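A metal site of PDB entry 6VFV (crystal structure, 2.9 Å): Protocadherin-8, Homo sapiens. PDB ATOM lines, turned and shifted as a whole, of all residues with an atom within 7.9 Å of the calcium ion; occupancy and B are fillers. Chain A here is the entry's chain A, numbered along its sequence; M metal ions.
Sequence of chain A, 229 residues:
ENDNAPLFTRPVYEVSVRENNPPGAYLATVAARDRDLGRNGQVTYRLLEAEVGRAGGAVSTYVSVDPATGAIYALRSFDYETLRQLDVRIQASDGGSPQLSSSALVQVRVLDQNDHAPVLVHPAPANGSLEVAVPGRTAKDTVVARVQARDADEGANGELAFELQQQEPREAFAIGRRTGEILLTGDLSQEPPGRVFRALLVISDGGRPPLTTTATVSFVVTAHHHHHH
The calcium ion is bound by the side-chain amide oxygen (OD1) of Asn 2 (2.2 Å). OD2 of Asp 34 binds the calcium ion. O of Asn 40 is bound to the calcium ion, 2.4 Å away. The backbone carbonyl oxygen (O) of Asn 4 is bound to the calcium ion (2.5 Å). The calcium ion is bound by OD1 of Asp 34, 2.5 Å away. The calcium ion is bound by OD1 of Asp 36 (2.5 Å). OD2 of Asp 94 binds the calcium ion (2.7 Å). The calcium ion has seven donor atoms within binding distance.
Of the 25 residues printed, 6 come within 4 Å of the calcium ion. The nearest printed residue that does not touch the calcium ion is Gly 41 (4.5 Å).
The backbone carbonyl oxygen (O) of Pro 98 lies within hydrogen-bond range of the side-chain amide nitrogen (ND2) of Asn 2 (3.4 Å). The side-chain amide oxygen of Asn 4 lies close to the side-chain carboxylate of Asp 3. OD1 of Asn 4 lies close to O of Arg 35, 3.2 Å away. The side-chain carboxylate of Asp 94 lies within hydrogen-bond range of the backbone NH of Leu 100. The side-chain carboxylate (OD1) of Asp 94 sits at hydrogen-bond distance from the backbone NH (N) of Gly 96, 3.3 Å away. NE2 of Gln 99 is in hydrogen-bond range of O of Asp 94, 2.9 Å away.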
ATOM      1  N   GLU A   1     -19.482 -24.631 -12.098  1.00  0.00           N
ATOM      2  CA  GLU A   1     -18.001 -24.483 -12.254  1.00  0.00           C
ATOM      3  C   GLU A   1     -17.674 -23.628 -13.473  1.00  0.00           C
ATOM      4  O   GLU A   1     -18.562 -23.084 -14.128  1.00  0.00           O
ATOM      5  CB  GLU A   1     -17.335 -25.861 -12.396  1.00  0.00           C
ATOM      6  CG  GLU A   1     -17.404 -26.727 -11.134  1.00  0.00           C
ATOM      7  CD  GLU A   1     -16.766 -28.086 -11.325  1.00  0.00           C
ATOM      8  OE1 GLU A   1     -16.412 -28.440 -12.472  1.00  0.00           O
ATOM      9  OE2 GLU A   1     -16.596 -28.808 -10.312  1.00  0.00           O
ATOM     10  N   ASN A   2     -16.372 -23.503 -13.749  1.00  0.00           N
ATOM     11  CA  ASN A   2     -15.885 -22.766 -14.917  1.00  0.00           C
ATOM     12  C   ASN A   2     -15.660 -23.747 -16.068  1.00  0.00           C
ATOM     13  O   ASN A   2     -14.536 -24.047 -16.474  1.00  0.00           O
ATOM     14  CB  ASN A   2     -14.610 -22.015 -14.556  1.00  0.00           C
ATOM     15  CG  ASN A   2     -14.096 -21.166 -15.704  1.00  0.00           C
ATOM     16  OD1 ASN A   2     -14.838 -20.848 -16.626  1.00  0.00           O
ATOM     17  ND2 ASN A   2     -12.826 -20.808 -15.642  1.00  0.00           N
ATOM     18  N   ASP A   3     -16.785 -24.251 -16.593  1.00  0.00           N
ATOM     19  CA  ASP A   3     -16.776 -25.290 -17.617  1.00  0.00           C
ATOM     20  C   ASP A   3     -17.039 -24.734 -19.008  1.00  0.00           C
ATOM     21  O   ASP A   3     -17.582 -25.434 -19.872  1.00  0.00           O
ATOM     22  CB  ASP A   3     -17.785 -26.375 -17.262  1.00  0.00           C
ATOM     23  CG  ASP A   3     -19.078 -25.824 -16.697  1.00  0.00           C
ATOM     24  OD1 ASP A   3     -19.562 -24.795 -17.224  1.00  0.00           O
ATOM     25  OD2 ASP A   3     -19.597 -26.394 -15.715  1.00  0.00           O
ATOM     26  N   ASN A   4     -16.661 -23.481 -19.263  1.00  0.00           N
ATOM     27  CA  ASN A   4     -16.764 -22.872 -20.580  1.00  0.00           C
ATOM     28  C   ASN A   4     -15.658 -21.831 -20.713  1.00  0.00           C
ATOM     29  O   ASN A   4     -15.587 -20.917 -19.894  1.00  0.00           O
ATOM     30  CB  ASN A   4     -18.122 -22.224 -20.801  1.00  0.00           C
ATOM     31  CG  ASN A   4     -19.223 -23.230 -21.010  1.00  0.00           C
ATOM     32  OD1 ASN A   4     -19.996 -23.524 -20.096  1.00  0.00           O
ATOM     33  ND2 ASN A   4     -19.320 -23.757 -22.228  1.00  0.00           N
ATOM     34  N   ALA A   5     -14.823 -21.973 -21.726  1.00  0.00           N
ATOM     35  CA  ALA A   5     -13.801 -20.979 -22.001  1.00  0.00           C
ATOM     36  C   ALA A   5     -14.390 -19.854 -22.840  1.00  0.00           C
ATOM     37  O   ALA A   5     -15.494 -19.970 -23.368  1.00  0.00           O
ATOM     38  CB  ALA A   5     -12.618 -21.622 -22.709  1.00  0.00           C
ATOM     39  N   PRO A   6     -13.675 -18.735 -22.975  1.00  0.00           N
ATOM     40  CA  PRO A   6     -14.155 -17.650 -23.850  1.00  0.00           C
ATOM     41  C   PRO A   6     -13.976 -18.007 -25.318  1.00  0.00           C
ATOM     42  O   PRO A   6     -12.858 -18.210 -25.783  1.00  0.00           O
ATOM     43  CB  PRO A   6     -13.291 -16.451 -23.449  1.00  0.00           C
ATOM     44  CG  PRO A   6     -12.711 -16.810 -22.112  1.00  0.00           C
ATOM     45  CD  PRO A   6     -12.548 -18.297 -22.146  1.00  0.00           C
ATOM     46  N   ARG A  33     -17.141 -14.709 -25.723  1.00  0.00           N
ATOM     47  CA  ARG A  33     -18.321 -15.049 -24.947  1.00  0.00           C
ATOM     48  C   ARG A  33     -17.965 -16.113 -23.930  1.00  0.00           C
ATOM     49  O   ARG A  33     -17.340 -17.122 -24.279  1.00  0.00           O
ATOM     50  CB  ARG A  33     -19.444 -15.559 -25.857  1.00  0.00           C
ATOM     51  CG  ARG A  33     -19.700 -14.710 -27.090  1.00  0.00           C
ATOM     52  CD  ARG A  33     -20.773 -13.678 -26.844  1.00  0.00           C
ATOM     53  NE  ARG A  33     -20.942 -12.831 -28.021  1.00  0.00           N
ATOM     54  CZ  ARG A  33     -20.781 -11.506 -28.052  1.00  0.00           C
ATOM     55  NH1 ARG A  33     -20.468 -10.819 -26.956  1.00  0.00           N
ATOM     56  NH2 ARG A  33     -20.964 -10.846 -29.195  1.00  0.00           N
ATOM     57  N   ASP A  34     -18.354 -15.892 -22.684  1.00  0.00           N
ATOM     58  CA  ASP A  34     -18.219 -16.898 -21.633  1.00  0.00           C
ATOM     59  C   ASP A  34     -19.604 -17.214 -21.091  1.00  0.00           C
ATOM     60  O   ASP A  34     -20.199 -16.406 -20.378  1.00  0.00           O
ATOM     61  CB  ASP A  34     -17.270 -16.429 -20.516  1.00  0.00           C
ATOM     62  CG  ASP A  34     -16.528 -17.595 -19.896  1.00  0.00           C
ATOM     63  OD1 ASP A  34     -15.296 -17.531 -19.757  1.00  0.00           O
ATOM     64  OD2 ASP A  34     -17.201 -18.592 -19.561  1.00  0.00           O
ATOM     65  N   ARG A  35     -20.110 -18.391 -21.445  1.00  0.00           N
ATOM     66  CA  ARG A  35     -21.412 -18.864 -20.980  1.00  0.00           C
ATOM     67  C   ARG A  35     -21.240 -19.511 -19.606  1.00  0.00           C
ATOM     68  O   ARG A  35     -21.427 -20.714 -19.411  1.00  0.00           O
ATOM     69  CB  ARG A  35     -22.008 -19.797 -22.020  1.00  0.00           C
ATOM     70  CG  ARG A  35     -23.111 -20.745 -21.553  1.00  0.00           C
ATOM     71  CD  ARG A  35     -22.871 -22.093 -22.187  1.00  0.00           C
ATOM     72  NE  ARG A  35     -22.517 -21.935 -23.595  1.00  0.00           N
ATOM     73  CZ  ARG A  35     -23.415 -21.830 -24.571  1.00  0.00           C
ATOM     74  NH1 ARG A  35     -24.701 -21.900 -24.301  1.00  0.00           N
ATOM     75  NH2 ARG A  35     -23.013 -21.672 -25.831  1.00  0.00           N
ATOM     76  N   ASP A  36     -20.860 -18.678 -18.645  1.00  0.00           N
ATOM     77  CA  ASP A  36     -20.837 -19.059 -17.242  1.00  0.00           C
ATOM     78  C   ASP A  36     -21.338 -17.872 -16.426  1.00  0.00           C
ATOM     79  O   ASP A  36     -21.093 -16.716 -16.775  1.00  0.00           O
ATOM     80  CB  ASP A  36     -19.425 -19.467 -16.749  1.00  0.00           C
ATOM     81  CG  ASP A  36     -18.887 -20.736 -17.429  1.00  0.00           C
ATOM     82  OD1 ASP A  36     -17.668 -20.785 -17.714  1.00  0.00           O
ATOM     83  OD2 ASP A  36     -19.668 -21.697 -17.660  1.00  0.00           O
ATOM     84  N   LEU A  37     -22.054 -18.169 -15.344  1.00  0.00           N
ATOM     85  CA  LEU A  37     -22.632 -17.116 -14.526  1.00  0.00           C
ATOM     86  C   LEU A  37     -21.618 -16.614 -13.510  1.00  0.00           C
ATOM     87  O   LEU A  37     -20.806 -17.393 -12.993  1.00  0.00           O
ATOM     88  CB  LEU A  37     -23.892 -17.617 -13.807  1.00  0.00           C
ATOM     89  CG  LEU A  37     -25.071 -17.966 -14.730  1.00  0.00           C
ATOM     90  CD1 LEU A  37     -26.230 -18.537 -13.930  1.00  0.00           C
ATOM     91  CD2 LEU A  37     -25.522 -16.741 -15.525  1.00  0.00           C
ATOM     92  N   GLY A  38     -21.651 -15.316 -13.239  1.00  0.00           N
ATOM     93  CA  GLY A  38     -20.774 -14.730 -12.251  1.00  0.00           C
ATOM     94  C   GLY A  38     -19.361 -14.524 -12.758  1.00  0.00           C
ATOM     95  O   GLY A  38     -19.126 -14.280 -13.943  1.00  0.00           O
ATOM     96  N   ARG A  39     -18.408 -14.640 -11.833  1.00  0.00           N
ATOM     97  CA  ARG A  39     -17.008 -14.359 -12.146  1.00  0.00           C
ATOM     98  C   ARG A  39     -16.430 -15.399 -13.096  1.00  0.00           C
ATOM     99  O   ARG A  39     -15.519 -15.092 -13.874  1.00  0.00           O
ATOM    100  CB  ARG A  39     -16.193 -14.301 -10.864  1.00  0.00           C
ATOM    101  CG  ARG A  39     -14.734 -13.922 -11.044  1.00  0.00           C
ATOM    102  CD  ARG A  39     -13.996 -13.938  -9.713  1.00  0.00           C
ATOM    103  NE  ARG A  39     -13.905 -15.289  -9.167  1.00  0.00           N
ATOM    104  CZ  ARG A  39     -13.547 -15.570  -7.916  1.00  0.00           C
ATOM    105  NH1 ARG A  39     -13.244 -14.584  -7.065  1.00  0.00           N
ATOM    106  NH2 ARG A  39     -13.485 -16.829  -7.504  1.00  0.00           N
ATOM    107  N   ASN A  40     -16.944 -16.636 -13.052  1.00  0.00           N
ATOM    108  CA  ASN A  40     -16.540 -17.626 -14.039  1.00  0.00           C
ATOM    109  C   ASN A  40     -16.804 -17.135 -15.459  1.00  0.00           C
ATOM    110  O   ASN A  40     -16.173 -17.624 -16.387  1.00  0.00           O
ATOM    111  CB  ASN A  40     -17.283 -18.949 -13.803  1.00  0.00           C
ATOM    112  CG  ASN A  40     -16.855 -19.645 -12.521  1.00  0.00           C
ATOM    113  OD1 ASN A  40     -15.660 -19.814 -12.258  1.00  0.00           O
ATOM    114  ND2 ASN A  40     -17.827 -20.068 -11.724  1.00  0.00           N
ATOM    115  N   GLY A  41     -17.705 -16.166 -15.622  1.00  0.00           N
ATOM    116  CA  GLY A  41     -18.078 -15.684 -16.936  1.00  0.00           C
ATOM    117  C   GLY A  41     -17.670 -14.265 -17.260  1.00  0.00           C
ATOM    118  O   GLY A  41     -18.017 -13.749 -18.325  1.00  0.00           O
ATOM    119  N   GLN A  42     -16.957 -13.596 -16.353  1.00  0.00           N
ATOM    120  CA  GLN A  42     -16.441 -12.264 -16.651  1.00  0.00           C
ATOM    121  C   GLN A  42     -15.114 -12.414 -17.390  1.00  0.00           C
ATOM    122  O   GLN A  42     -14.153 -12.982 -16.851  1.00  0.00           O
ATOM    123  CB  GLN A  42     -16.288 -11.444 -15.375  1.00  0.00           C
ATOM    124  CG  GLN A  42     -15.125 -11.822 -14.465  1.00  0.00           C
ATOM    125  CD  GLN A  42     -15.063 -10.990 -13.202  1.00  0.00           C
ATOM    126  OE1 GLN A  42     -16.065 -10.409 -12.778  1.00  0.00           O
ATOM    127  NE2 GLN A  42     -13.882 -10.904 -12.595  1.00  0.00           N
ATOM    128  N   VAL A  43     -15.061 -11.920 -18.625  1.00  0.00           N
ATOM    129  CA  VAL A  43     -13.902 -12.090 -19.492  1.00  0.00           C
ATOM    130  C   VAL A  43     -13.148 -10.775 -19.605  1.00  0.00           C
ATOM    131  O   VAL A  43     -13.759  -9.699 -19.641  1.00  0.00           O
ATOM    132  CB  VAL A  43     -14.317 -12.622 -20.884  1.00  0.00           C
ATOM    133  CG1 VAL A  43     -15.254 -11.658 -21.578  1.00  0.00           C
ATOM    134  CG2 VAL A  43     -13.090 -12.880 -21.739  1.00  0.00           C
ATOM    135  N   SER A  93      -9.749 -13.936 -21.572  1.00  0.00           N
ATOM    136  CA  SER A  93      -9.455 -14.789 -20.431  1.00  0.00           C
ATOM    137  C   SER A  93     -10.436 -14.496 -19.305  1.00  0.00           C
ATOM    138  O   SER A  93     -10.595 -13.347 -18.914  1.00  0.00           O
ATOM    139  CB  SER A  93      -8.014 -14.575 -19.962  1.00  0.00           C
ATOM    140  OG  SER A  93      -7.694 -15.430 -18.882  1.00  0.00           O
ATOM    141  N   ASP A  94     -11.061 -15.550 -18.765  1.00  0.00           N
ATOM    142  CA  ASP A  94     -12.091 -15.381 -17.746  1.00  0.00           C
ATOM    143  C   ASP A  94     -11.456 -15.215 -16.363  1.00  0.00           C
ATOM    144  O   ASP A  94     -10.240 -15.104 -16.213  1.00  0.00           O
ATOM    145  CB  ASP A  94     -13.068 -16.551 -17.783  1.00  0.00           C
ATOM    146  CG  ASP A  94     -12.417 -17.884 -17.449  1.00  0.00           C
ATOM    147  OD1 ASP A  94     -11.384 -17.904 -16.743  1.00  0.00           O
ATOM    148  OD2 ASP A  94     -12.961 -18.921 -17.883  1.00  0.00           O
ATOM    149  N   GLY A  95     -12.298 -15.226 -15.328  1.00  0.00           N
ATOM    150  CA  GLY A  95     -11.838 -15.014 -13.964  1.00  0.00           C
ATOM    151  C   GLY A  95     -12.101 -16.172 -13.037  1.00  0.00           C
ATOM    152  O   GLY A  95     -12.291 -15.992 -11.822  1.00  0.00           O
ATOM    153  N   GLY A  96     -12.122 -17.395 -13.592  1.00  0.00           N
ATOM    154  CA  GLY A  96     -12.290 -18.592 -12.794  1.00  0.00           C
ATOM    155  C   GLY A  96     -10.951 -19.149 -12.323  1.00  0.00           C
ATOM    156  O   GLY A  96      -9.877 -18.636 -12.646  1.00  0.00           O
ATOM    157  N   PRO A  98      -8.886 -22.753 -12.268  1.00  0.00           N
ATOM    158  CA  PRO A  98      -7.925 -21.953 -13.040  1.00  0.00           C
ATOM    159  C   PRO A  98      -8.566 -21.155 -14.174  1.00  0.00           C
ATOM    160  O   PRO A  98      -9.679 -21.462 -14.607  1.00  0.00           O
ATOM    161  CB  PRO A  98      -6.965 -23.004 -13.598  1.00  0.00           C
ATOM    162  CG  PRO A  98      -7.807 -24.220 -13.754  1.00  0.00           C
ATOM    163  CD  PRO A  98      -8.783 -24.193 -12.603  1.00  0.00           C
ATOM    164  N   GLN A  99      -7.864 -20.130 -14.645  1.00  0.00           N
ATOM    165  CA  GLN A  99      -8.350 -19.311 -15.744  1.00  0.00           C
ATOM    166  C   GLN A  99      -8.392 -20.124 -17.032  1.00  0.00           C
ATOM    167  O   GLN A  99      -7.501 -20.933 -17.304  1.00  0.00           O
ATOM    168  CB  GLN A  99      -7.460 -18.085 -15.934  1.00  0.00           C
ATOM    169  CG  GLN A  99      -7.844 -16.881 -15.087  1.00  0.00           C
ATOM    170  CD  GLN A  99      -6.985 -15.665 -15.375  1.00  0.00           C
ATOM    171  OE1 GLN A  99      -5.822 -15.778 -15.762  1.00  0.00           O
ATOM    172  NE2 GLN A  99      -7.555 -14.472 -15.192  1.00  0.00           N
ATOM    173  N   LEU A 100      -9.429 -19.885 -17.826  1.00  0.00           N
ATOM    174  CA  LEU A 100      -9.515 -20.405 -19.186  1.00  0.00           C
ATOM    175  C   LEU A 100      -9.399 -19.252 -20.164  1.00  0.00           C
ATOM    176  O   LEU A 100      -9.925 -18.154 -19.911  1.00  0.00           O
ATOM    177  CB  LEU A 100     -10.833 -21.155 -19.404  1.00  0.00           C
ATOM    178  CG  LEU A 100     -11.070 -22.359 -18.487  1.00  0.00           C
ATOM    179  CD1 LEU A 100     -12.410 -23.004 -18.803  1.00  0.00           C
ATOM    180  CD2 LEU A 100      -9.938 -23.373 -18.612  1.00  0.00           C
ATOM    181  N   SER A 101      -8.717 -19.489 -21.283  1.00  0.00           N
ATOM    182  CA  SER A 101      -8.386 -18.407 -22.205  1.00  0.00           C
ATOM    183  C   SER A 101      -8.458 -18.906 -23.641  1.00  0.00           C
ATOM    184  O   SER A 101      -8.394 -20.106 -23.917  1.00  0.00           O
ATOM    185  CB  SER A 101      -6.996 -17.832 -21.915  1.00  0.00           C
ATOM    186  OG  SER A 101      -6.026 -18.861 -21.773  1.00  0.00           O
HETATM  187 CA    CA M   1     -15.632 -19.299 -18.051  1.00  0.00          CA
